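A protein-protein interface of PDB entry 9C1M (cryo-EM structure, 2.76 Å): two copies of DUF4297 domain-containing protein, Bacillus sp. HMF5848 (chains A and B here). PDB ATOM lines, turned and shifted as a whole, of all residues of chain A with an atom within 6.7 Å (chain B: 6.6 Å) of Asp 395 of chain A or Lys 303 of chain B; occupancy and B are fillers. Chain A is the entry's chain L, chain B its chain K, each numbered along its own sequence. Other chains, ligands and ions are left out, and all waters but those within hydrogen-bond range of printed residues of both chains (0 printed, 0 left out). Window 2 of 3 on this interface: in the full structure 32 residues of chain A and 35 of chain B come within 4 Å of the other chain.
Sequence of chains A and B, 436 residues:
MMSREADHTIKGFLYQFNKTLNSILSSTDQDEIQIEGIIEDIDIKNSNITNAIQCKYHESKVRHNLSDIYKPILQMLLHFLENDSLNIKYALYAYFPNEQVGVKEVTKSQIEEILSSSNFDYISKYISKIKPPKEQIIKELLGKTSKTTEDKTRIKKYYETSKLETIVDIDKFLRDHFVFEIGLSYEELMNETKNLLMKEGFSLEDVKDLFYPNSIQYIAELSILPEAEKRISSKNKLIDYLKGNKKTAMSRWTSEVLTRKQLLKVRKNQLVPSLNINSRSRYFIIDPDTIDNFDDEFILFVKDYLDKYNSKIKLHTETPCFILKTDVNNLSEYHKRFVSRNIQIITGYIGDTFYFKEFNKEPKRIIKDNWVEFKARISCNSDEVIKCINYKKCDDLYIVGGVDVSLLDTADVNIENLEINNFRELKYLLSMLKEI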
ATOM      1  N   SER A 279      10.119  13.752  -4.548  1.00  0.00           N
ATOM      2  CA  SER A 279       9.961  12.364  -4.118  1.00  0.00           C
ATOM      3  C   SER A 279      11.185  11.549  -4.508  1.00  0.00           C
ATOM      4  O   SER A 279      11.089  10.458  -5.075  1.00  0.00           O
ATOM      5  CB  SER A 279       8.692  11.754  -4.706  1.00  0.00           C
ATOM      6  OG  SER A 279       7.537  12.413  -4.218  1.00  0.00           O
ATOM      7  N   ARG A 280      12.365  12.080  -4.204  1.00  0.00           N
ATOM      8  CA  ARG A 280      13.628  11.463  -4.581  1.00  0.00           C
ATOM      9  C   ARG A 280      14.414  11.035  -3.351  1.00  0.00           C
ATOM     10  O   ARG A 280      14.584  11.816  -2.409  1.00  0.00           O
ATOM     11  CB  ARG A 280      14.453  12.412  -5.455  1.00  0.00           C
ATOM     12  CG  ARG A 280      15.744  11.795  -5.908  1.00  0.00           C
ATOM     13  CD  ARG A 280      15.481  10.629  -6.822  1.00  0.00           C
ATOM     14  NE  ARG A 280      14.740  10.904  -8.045  1.00  0.00           N
ATOM     15  CZ  ARG A 280      15.292  11.346  -9.166  1.00  0.00           C
ATOM     16  NH1 ARG A 280      16.584  11.619  -9.237  1.00  0.00           N
ATOM     17  NH2 ARG A 280      14.537  11.488 -10.249  1.00  0.00           N
ATOM     18  N   SER A 281      14.888   9.789  -3.370  1.00  0.00           N
ATOM     19  CA  SER A 281      15.719   9.242  -2.304  1.00  0.00           C
ATOM     20  C   SER A 281      17.184   9.458  -2.659  1.00  0.00           C
ATOM     21  O   SER A 281      17.670   8.928  -3.665  1.00  0.00           O
ATOM     22  CB  SER A 281      15.428   7.756  -2.100  1.00  0.00           C
ATOM     23  OG  SER A 281      15.625   7.027  -3.300  1.00  0.00           O
ATOM     24  N   ARG A 282      17.886  10.228  -1.833  1.00  0.00           N
ATOM     25  CA  ARG A 282      19.260  10.632  -2.098  1.00  0.00           C
ATOM     26  C   ARG A 282      20.162  10.124  -0.983  1.00  0.00           C
ATOM     27  O   ARG A 282      19.858  10.313   0.199  1.00  0.00           O
ATOM     28  CB  ARG A 282      19.355  12.155  -2.215  1.00  0.00           C
ATOM     29  CG  ARG A 282      18.310  12.751  -3.140  1.00  0.00           C
ATOM     30  CD  ARG A 282      18.391  14.264  -3.191  1.00  0.00           C
ATOM     31  NE  ARG A 282      17.315  14.830  -3.993  1.00  0.00           N
ATOM     32  CZ  ARG A 282      16.165  15.271  -3.502  1.00  0.00           C
ATOM     33  NH1 ARG A 282      15.906  15.223  -2.205  1.00  0.00           N
ATOM     34  NH2 ARG A 282      15.252  15.768  -4.329  1.00  0.00           N
ATOM     35  N   TYR A 283      21.261   9.479  -1.361  1.00  0.00           N
ATOM     36  CA  TYR A 283      22.232   8.943  -0.414  1.00  0.00           C
ATOM     37  C   TYR A 283      23.542   9.707  -0.552  1.00  0.00           C
ATOM     38  O   TYR A 283      24.025   9.921  -1.669  1.00  0.00           O
ATOM     39  CB  TYR A 283      22.470   7.448  -0.641  1.00  0.00           C
ATOM     40  CG  TYR A 283      21.315   6.541  -0.259  1.00  0.00           C
ATOM     41  CD1 TYR A 283      20.087   7.058   0.125  1.00  0.00           C
ATOM     42  CD2 TYR A 283      21.461   5.163  -0.281  1.00  0.00           C
ATOM     43  CE1 TYR A 283      19.038   6.230   0.472  1.00  0.00           C
ATOM     44  CE2 TYR A 283      20.417   4.327   0.062  1.00  0.00           C
ATOM     45  CZ  TYR A 283      19.208   4.865   0.439  1.00  0.00           C
ATOM     46  OH  TYR A 283      18.168   4.034   0.783  1.00  0.00           O
ATOM     47  N   GLU A 318      10.599  11.149   0.997  1.00  0.00           N
ATOM     48  CA  GLU A 318      11.790  10.311   1.069  1.00  0.00           C
ATOM     49  C   GLU A 318      12.761  10.874   2.097  1.00  0.00           C
ATOM     50  O   GLU A 318      13.013  12.083   2.125  1.00  0.00           O
ATOM     51  CB  GLU A 318      12.467  10.202  -0.299  1.00  0.00           C
ATOM     52  CG  GLU A 318      11.574   9.622  -1.381  1.00  0.00           C
ATOM     53  CD  GLU A 318      10.898   8.336  -0.945  1.00  0.00           C
ATOM     54  OE1 GLU A 318      11.613   7.349  -0.671  1.00  0.00           O
ATOM     55  OE2 GLU A 318       9.650   8.312  -0.874  1.00  0.00           O
ATOM     56  N   LYS A 393      18.057   0.181  -2.740  1.00  0.00           N
ATOM     57  CA  LYS A 393      18.830   1.036  -3.630  1.00  0.00           C
ATOM     58  C   LYS A 393      18.211   2.424  -3.724  1.00  0.00           C
ATOM     59  O   LYS A 393      16.987   2.579  -3.753  1.00  0.00           O
ATOM     60  CB  LYS A 393      18.926   0.413  -5.021  1.00  0.00           C
ATOM     61  CG  LYS A 393      20.230  -0.320  -5.282  1.00  0.00           C
ATOM     62  CD  LYS A 393      20.046  -1.445  -6.285  1.00  0.00           C
ATOM     63  CE  LYS A 393      21.378  -1.872  -6.875  1.00  0.00           C
ATOM     64  NZ  LYS A 393      21.206  -2.744  -8.070  1.00  0.00           N
ATOM     65  N   CYS A 394      19.071   3.436  -3.770  1.00  0.00           N
ATOM     66  CA  CYS A 394      18.639   4.814  -3.914  1.00  0.00           C
ATOM     67  C   CYS A 394      18.495   5.160  -5.394  1.00  0.00           C
ATOM     68  O   CYS A 394      18.804   4.361  -6.281  1.00  0.00           O
ATOM     69  CB  CYS A 394      19.624   5.759  -3.230  1.00  0.00           C
ATOM     70  SG  CYS A 394      21.344   5.514  -3.728  1.00  0.00           S
ATOM     71  N   ASP A 395      18.022   6.372  -5.664  1.00  0.00           N
ATOM     72  CA  ASP A 395      17.925   6.859  -7.032  1.00  0.00           C
ATOM     73  C   ASP A 395      19.084   7.762  -7.419  1.00  0.00           C
ATOM     74  O   ASP A 395      19.466   7.797  -8.593  1.00  0.00           O
ATOM     75  CB  ASP A 395      16.611   7.613  -7.230  1.00  0.00           C
ATOM     76  CG  ASP A 395      15.395   6.711  -7.179  1.00  0.00           C
ATOM     77  OD1 ASP A 395      15.510   5.521  -7.534  1.00  0.00           O
ATOM     78  OD2 ASP A 395      14.316   7.199  -6.780  1.00  0.00           O
ATOM     79  N   ASP A 396      19.644   8.494  -6.460  1.00  0.00           N
ATOM     80  CA  ASP A 396      20.843   9.293  -6.659  1.00  0.00           C
ATOM     81  C   ASP A 396      21.842   8.946  -5.568  1.00  0.00           C
ATOM     82  O   ASP A 396      21.467   8.775  -4.404  1.00  0.00           O
ATOM     83  CB  ASP A 396      20.532  10.793  -6.636  1.00  0.00           C
ATOM     84  CG  ASP A 396      19.860  11.269  -7.906  1.00  0.00           C
ATOM     85  OD1 ASP A 396      20.320  10.888  -9.003  1.00  0.00           O
ATOM     86  OD2 ASP A 396      18.871  12.026  -7.810  1.00  0.00           O
ATOM     87  N   LEU A 397      23.114   8.835  -5.946  1.00  0.00           N
ATOM     88  CA  LEU A 397      24.180   8.462  -5.018  1.00  0.00           C
ATOM     89  C   LEU A 397      25.311   9.476  -5.157  1.00  0.00           C
ATOM     90  O   LEU A 397      26.104   9.408  -6.102  1.00  0.00           O
ATOM     91  CB  LEU A 397      24.667   7.041  -5.285  1.00  0.00           C
ATOM     92  CG  LEU A 397      25.740   6.498  -4.341  1.00  0.00           C
ATOM     93  CD1 LEU A 397      25.255   6.533  -2.903  1.00  0.00           C
ATOM     94  CD2 LEU A 397      26.135   5.086  -4.741  1.00  0.00           C
ATOM     95  N   ASP A 412      22.739   0.240 -12.000  1.00  0.00           N
ATOM     96  CA  ASP A 412      21.457   0.919 -12.197  1.00  0.00           C
ATOM     97  C   ASP A 412      21.158   1.938 -11.099  1.00  0.00           C
ATOM     98  O   ASP A 412      20.003   2.124 -10.710  1.00  0.00           O
ATOM     99  CB  ASP A 412      20.312  -0.092 -12.309  1.00  0.00           C
ATOM    100  CG  ASP A 412      20.381  -0.905 -13.586  1.00  0.00           C
ATOM    101  OD1 ASP A 412      20.901  -0.388 -14.596  1.00  0.00           O
ATOM    102  OD2 ASP A 412      19.918  -2.065 -13.579  1.00  0.00           O
ATOM    103  N   VAL A 413      22.189   2.610 -10.590  1.00  0.00           N
ATOM    104  CA  VAL A 413      22.023   3.725  -9.666  1.00  0.00           C
ATOM    105  C   VAL A 413      22.811   4.913 -10.201  1.00  0.00           C
ATOM    106  O   VAL A 413      23.932   4.756 -10.698  1.00  0.00           O
ATOM    107  CB  VAL A 413      22.458   3.367  -8.226  1.00  0.00           C
ATOM    108  CG1 VAL A 413      21.599   2.239  -7.677  1.00  0.00           C
ATOM    109  CG2 VAL A 413      23.927   2.989  -8.176  1.00  0.00           C
ATOM    110  N   ASN A 414      22.213   6.099 -10.123  1.00  0.00           N
ATOM    111  CA  ASN A 414      22.811   7.307 -10.686  1.00  0.00           C
ATOM    112  C   ASN A 414      23.886   7.809  -9.730  1.00  0.00           C
ATOM    113  O   ASN A 414      23.592   8.480  -8.739  1.00  0.00           O
ATOM    114  CB  ASN A 414      21.742   8.366 -10.932  1.00  0.00           C
ATOM    115  CG  ASN A 414      22.312   9.654 -11.494  1.00  0.00           C
ATOM    116  OD1 ASN A 414      23.410   9.673 -12.049  1.00  0.00           O
ATOM    117  ND2 ASN A 414      21.562  10.742 -11.356  1.00  0.00           N
ATOM    118  N   ILE A 415      25.140   7.484 -10.031  1.00  0.00           N
ATOM    119  CA  ILE A 415      26.276   7.916  -9.226  1.00  0.00           C
ATOM    120  C   ILE A 415      26.734   9.278  -9.724  1.00  0.00           C
ATOM    121  O   ILE A 415      26.925   9.478 -10.929  1.00  0.00           O
ATOM    122  CB  ILE A 415      27.420   6.893  -9.291  1.00  0.00           C
ATOM    123  CG1 ILE A 415      26.986   5.567  -8.669  1.00  0.00           C
ATOM    124  CG2 ILE A 415      28.657   7.427  -8.590  1.00  0.00           C
ATOM    125  CD1 ILE A 415      28.073   4.522  -8.657  1.00  0.00           C
ATOM    126  N   PHE B 298      20.600   1.918 -20.414  1.00  0.00           N
ATOM    127  CA  PHE B 298      19.228   1.847 -20.907  1.00  0.00           C
ATOM    128  C   PHE B 298      18.216   1.983 -19.773  1.00  0.00           C
ATOM    129  O   PHE B 298      17.188   2.650 -19.932  1.00  0.00           O
ATOM    130  CB  PHE B 298      19.010   0.539 -21.667  1.00  0.00           C
ATOM    131  CG  PHE B 298      17.638   0.409 -22.268  1.00  0.00           C
ATOM    132  CD1 PHE B 298      17.059   1.470 -22.940  1.00  0.00           C
ATOM    133  CD2 PHE B 298      16.929  -0.776 -22.159  1.00  0.00           C
ATOM    134  CE1 PHE B 298      15.798   1.354 -23.493  1.00  0.00           C
ATOM    135  CE2 PHE B 298      15.668  -0.896 -22.710  1.00  0.00           C
ATOM    136  CZ  PHE B 298      15.102   0.170 -23.377  1.00  0.00           C
ATOM    137  N   ILE B 299      18.485   1.353 -18.628  1.00  0.00           N
ATOM    138  CA  ILE B 299      17.528   1.367 -17.523  1.00  0.00           C
ATOM    139  C   ILE B 299      17.355   2.782 -16.982  1.00  0.00           C
ATOM    140  O   ILE B 299      16.231   3.242 -16.743  1.00  0.00           O
ATOM    141  CB  ILE B 299      17.974   0.396 -16.416  1.00  0.00           C
ATOM    142  CG1 ILE B 299      18.420  -0.940 -17.016  1.00  0.00           C
ATOM    143  CG2 ILE B 299      16.854   0.181 -15.413  1.00  0.00           C
ATOM    144  CD1 ILE B 299      17.325  -1.692 -17.727  1.00  0.00           C
ATOM    145  N   LEU B 300      18.468   3.492 -16.778  1.00  0.00           N
ATOM    146  CA  LEU B 300      18.404   4.834 -16.209  1.00  0.00           C
ATOM    147  C   LEU B 300      17.695   5.804 -17.147  1.00  0.00           C
ATOM    148  O   LEU B 300      16.948   6.682 -16.694  1.00  0.00           O
ATOM    149  CB  LEU B 300      19.811   5.331 -15.883  1.00  0.00           C
ATOM    150  CG  LEU B 300      20.611   4.468 -14.905  1.00  0.00           C
ATOM    151  CD1 LEU B 300      22.052   4.945 -14.817  1.00  0.00           C
ATOM    152  CD2 LEU B 300      19.959   4.467 -13.531  1.00  0.00           C
ATOM    153  N   PHE B 301      17.930   5.674 -18.456  1.00  0.00           N
ATOM    154  CA  PHE B 301      17.251   6.539 -19.415  1.00  0.00           C
ATOM    155  C   PHE B 301      15.741   6.351 -19.352  1.00  0.00           C
ATOM    156  O   PHE B 301      14.986   7.330 -19.343  1.00  0.00           O
ATOM    157  CB  PHE B 301      17.767   6.265 -20.829  1.00  0.00           C
ATOM    158  CG  PHE B 301      16.930   6.886 -21.910  1.00  0.00           C
ATOM    159  CD1 PHE B 301      17.051   8.230 -22.212  1.00  0.00           C
ATOM    160  CD2 PHE B 301      16.025   6.123 -22.629  1.00  0.00           C
ATOM    161  CE1 PHE B 301      16.283   8.804 -23.206  1.00  0.00           C
ATOM    162  CE2 PHE B 301      15.255   6.693 -23.625  1.00  0.00           C
ATOM    163  CZ  PHE B 301      15.385   8.034 -23.912  1.00  0.00           C
ATOM    164  N   VAL B 302      15.283   5.098 -19.293  1.00  0.00           N
ATOM    165  CA  VAL B 302      13.850   4.835 -19.208  1.00  0.00           C
ATOM    166  C   VAL B 302      13.292   5.341 -17.884  1.00  0.00           C
ATOM    167  O   VAL B 302      12.178   5.876 -17.830  1.00  0.00           O
ATOM    168  CB  VAL B 302      13.570   3.335 -19.411  1.00  0.00           C
ATOM    169  CG1 VAL B 302      12.091   3.035 -19.216  1.00  0.00           C
ATOM    170  CG2 VAL B 302      14.024   2.897 -20.790  1.00  0.00           C
ATOM    171  N   LYS B 303      14.051   5.182 -16.796  1.00  0.00           N
ATOM    172  CA  LYS B 303      13.584   5.667 -15.500  1.00  0.00           C
ATOM    173  C   LYS B 303      13.407   7.183 -15.508  1.00  0.00           C
ATOM    174  O   LYS B 303      12.396   7.701 -15.020  1.00  0.00           O
ATOM    175  CB  LYS B 303      14.558   5.241 -14.402  1.00  0.00           C
ATOM    176  CG  LYS B 303      13.998   5.360 -12.995  1.00  0.00           C
ATOM    177  CD  LYS B 303      15.046   5.008 -11.953  1.00  0.00           C
ATOM    178  CE  LYS B 303      15.155   6.087 -10.892  1.00  0.00           C
ATOM    179  NZ  LYS B 303      13.880   6.260 -10.146  1.00  0.00           N
ATOM    180  N   ASP B 304      14.376   7.909 -16.073  1.00  0.00           N
ATOM    181  CA  ASP B 304      14.248   9.362 -16.166  1.00  0.00           C
ATOM    182  C   ASP B 304      13.113   9.760 -17.102  1.00  0.00           C
ATOM    183  O   ASP B 304      12.395  10.735 -16.839  1.00  0.00           O
ATOM    184  CB  ASP B 304      15.570   9.977 -16.625  1.00  0.00           C
ATOM    185  CG  ASP B 304      16.660   9.862 -15.576  1.00  0.00           C
ATOM    186  OD1 ASP B 304      16.329   9.841 -14.372  1.00  0.00           O
ATOM    187  OD2 ASP B 304      17.847   9.795 -15.956  1.00  0.00           O
ATOM    188  N   TYR B 305      12.932   9.018 -18.198  1.00  0.00           N
ATOM    189  CA  TYR B 305      11.837   9.309 -19.116  1.00  0.00           C
ATOM    190  C   TYR B 305      10.488   9.142 -18.430  1.00  0.00           C
ATOM    191  O   TYR B 305       9.568   9.934 -18.656  1.00  0.00           O
ATOM    192  CB  TYR B 305      11.931   8.411 -20.350  1.00  0.00           C
ATOM    193  CG  TYR B 305      10.885   8.702 -21.405  1.00  0.00           C
ATOM    194  CD1 TYR B 305       9.628   8.115 -21.347  1.00  0.00           C
ATOM    195  CD2 TYR B 305      11.151   9.569 -22.453  1.00  0.00           C
ATOM    196  CE1 TYR B 305       8.669   8.381 -22.304  1.00  0.00           C
ATOM    197  CE2 TYR B 305      10.198   9.840 -23.414  1.00  0.00           C
ATOM    198  CZ  TYR B 305       8.960   9.243 -23.335  1.00  0.00           C
ATOM    199  OH  TYR B 305       8.007   9.511 -24.291  1.00  0.00           O
ATOM    200  N   LEU B 306      10.342   8.105 -17.604  1.00  0.00           N
ATOM    201  CA  LEU B 306       9.096   7.926 -16.867  1.00  0.00           C
ATOM    202  C   LEU B 306       8.936   8.970 -15.770  1.00  0.00           C
ATOM    203  O   LEU B 306       7.810   9.384 -15.473  1.00  0.00           O
ATOM    204  CB  LEU B 306       9.025   6.518 -16.279  1.00  0.00           C
ATOM    205  CG  LEU B 306       9.108   5.380 -17.295  1.00  0.00           C
ATOM    206  CD1 LEU B 306       9.041   4.035 -16.599  1.00  0.00           C
ATOM    207  CD2 LEU B 306       8.004   5.507 -18.331  1.00  0.00           C
ATOM    208  N   ASP B 307      10.041   9.402 -15.157  1.00  0.00           N
ATOM    209  CA  ASP B 307       9.960  10.471 -14.167  1.00  0.00           C
ATOM    210  C   ASP B 307       9.496  11.778 -14.795  1.00  0.00           C
ATOM    211  O   ASP B 307       8.801  12.566 -14.145  1.00  0.00           O
ATOM    212  CB  ASP B 307      11.315  10.663 -13.485  1.00  0.00           C
ATOM    213  CG  ASP B 307      11.464   9.818 -12.235  1.00  0.00           C
ATOM    214  OD1 ASP B 307      10.530   9.052 -11.918  1.00  0.00           O
ATOM    215  OD2 ASP B 307      12.515   9.921 -11.569  1.00  0.00           O
ATOM    216  N   LYS B 308       9.872  12.025 -16.048  1.00  0.00           N
ATOM    217  CA  LYS B 308       9.500  13.271 -16.711  1.00  0.00           C
ATOM    218  C   LYS B 308       8.133  13.214 -17.387  1.00  0.00           C
ATOM    219  O   LYS B 308       7.356  14.169 -17.285  1.00  0.00           O
ATOM    220  CB  LYS B 308      10.564  13.655 -17.743  1.00  0.00           C
ATOM    221  CG  LYS B 308      10.265  14.949 -18.488  1.00  0.00           C
ATOM    222  CD  LYS B 308      10.335  16.157 -17.573  1.00  0.00           C
ATOM    223  CE  LYS B 308      10.188  17.450 -18.360  1.00  0.00           C
ATOM    224  NZ  LYS B 308       8.830  17.579 -18.963  1.00  0.00           N
ATOM    225  N   PHE B 338      14.874  -4.391 -15.139  1.00  0.00           N
ATOM    226  CA  PHE B 338      13.783  -3.474 -14.827  1.00  0.00           C
ATOM    227  C   PHE B 338      13.009  -3.935 -13.597  1.00  0.00           C
ATOM    228  O   PHE B 338      12.583  -3.110 -12.779  1.00  0.00           O
ATOM    229  CB  PHE B 338      12.849  -3.333 -16.030  1.00  0.00           C
ATOM    230  CG  PHE B 338      13.274  -2.274 -17.008  1.00  0.00           C
ATOM    231  CD1 PHE B 338      13.180  -0.933 -16.682  1.00  0.00           C
ATOM    232  CD2 PHE B 338      13.766  -2.621 -18.254  1.00  0.00           C
ATOM    233  CE1 PHE B 338      13.570   0.040 -17.581  1.00  0.00           C
ATOM    234  CE2 PHE B 338      14.158  -1.653 -19.153  1.00  0.00           C
ATOM    235  CZ  PHE B 338      14.059  -0.320 -18.819  1.00  0.00           C
ATOM    236  N   ARG B 341      14.655  -2.998 -10.336  1.00  0.00           N
ATOM    237  CA  ARG B 341      14.615  -1.577 -10.027  1.00  0.00           C
ATOM    238  C   ARG B 341      13.191  -1.083  -9.760  1.00  0.00           C
ATOM    239  O   ARG B 341      12.974   0.122  -9.591  1.00  0.00           O
ATOM    240  CB  ARG B 341      15.295  -0.802 -11.165  1.00  0.00           C
ATOM    241  CG  ARG B 341      15.366   0.696 -10.989  1.00  0.00           C
ATOM    242  CD  ARG B 341      16.272   1.013  -9.825  1.00  0.00           C
ATOM    243  NE  ARG B 341      16.418   2.447  -9.633  1.00  0.00           N
ATOM    244  CZ  ARG B 341      17.019   3.001  -8.593  1.00  0.00           C
ATOM    245  NH1 ARG B 341      17.514   2.271  -7.608  1.00  0.00           N
ATOM    246  NH2 ARG B 341      17.117   4.323  -8.535  1.00  0.00           N
ATOM    247  N   ILE B 343      10.468  -1.076 -11.684  1.00  0.00           N
ATOM    248  CA  ILE B 343       9.813  -0.430 -12.816  1.00  0.00           C
ATOM    249  C   ILE B 343       8.965  -1.484 -13.511  1.00  0.00           C
ATOM    250  O   ILE B 343       9.482  -2.520 -13.946  1.00  0.00           O
ATOM    251  CB  ILE B 343      10.826   0.198 -13.785  1.00  0.00           C
ATOM    252  CG1 ILE B 343      11.863   1.021 -13.019  1.00  0.00           C
ATOM    253  CG2 ILE B 343      10.113   1.058 -14.814  1.00  0.00           C
ATOM    254  CD1 ILE B 343      13.029   1.475 -13.866  1.00  0.00           C
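No position is printed for both chains. Of the 8 pairs that touch across the chains among the printed residues, none has its exchanged pair printed and touching as well.
Lys 393 of chain A touches Arg 341 of chain B (CB to NH1, 3.5 Å). Ile 299 of chain B touches Asp 412 of chain A. O of Asp 412 of chain A touches CD2 of Leu 300 of chain B, 3.7 Å away. O of Asp 412 of chain A touches NE of Arg 341 of chain B, at 3.8 Å.
Printed residues of chain B that touch a printed residue of chain A: Ile 299, Leu 300, Lys 303, Asp 307 and Arg 341. Hydrophobic or aromatic side chains of chain B that line the printed part of chain A: Ile 299 and Leu 300. Among the printed residues, 8 pairs touch across the chains. Among the printed residues, Asp or Glu carboxylates within 4 Å of a Lys or Arg side-chain nitrogen of the other chain: Arg 280 of chain A with Asp 307 of chain B, Asp 395 of chain A with Lys 303 of chain B and Asp 395 of chain A with Arg 341 of chain B.
Arg 282 of chain A touches none of the printed residues of chain B. Tyr 283 of chain A touches none of the printed residues of chain B. Printed residues of chain B within 4 Å of Cys 394 of chain A: Arg 341 (2.8 Å). Of chain B, only Lys 303 (3.2 Å) and Arg 341 (2.2 Å) come within 4 Å of Asp 395 of chain A. Printed residues of chain A within 4 Å of Leu 300 of chain B: Asp 412 (3.7 Å). Lys 303 of chain B touches one residue of chain A. Printed residues of chain A within 4 Å of Asp 307 of chain B: Arg 280 (2.9 Å).
NZ of Lys 303 of chain B is in salt-bridge range of OD1 of Asp 395 of chain A, 3.2 Å away. NH2 of Arg 280 of chain A lies within salt-bridge range of OD2 of Asp 307 of chain B (2.9 Å). O of Cys 394 of chain A lies within hydrogen-bond range of NH1 of Arg 341 of chain B, at 2.8 Å. The guanidinium group (NH1) of Arg 341 of chain B lies within salt-bridge range of the side-chain carboxylate (OD1) of Asp 395 of chain A (3.8 Å).
NE of Arg 280 of chain A is in salt-bridge range of OD2 of Asp 395 of chain A, at 3.9 Å. NH1 of Arg 280 of chain A is in salt-bridge range of OD2 of Asp 396 of chain A (2.7 Å). The backbone carbonyl oxygen (O) of Ser 281 of chain A is in hydrogen-bond range of the backbone NH (N) of Asp 395 of chain A (3.3 Å). O of Asp 396 of chain A is in hydrogen-bond range of SG of Cys 394 of chain A, at 3.3 Å.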
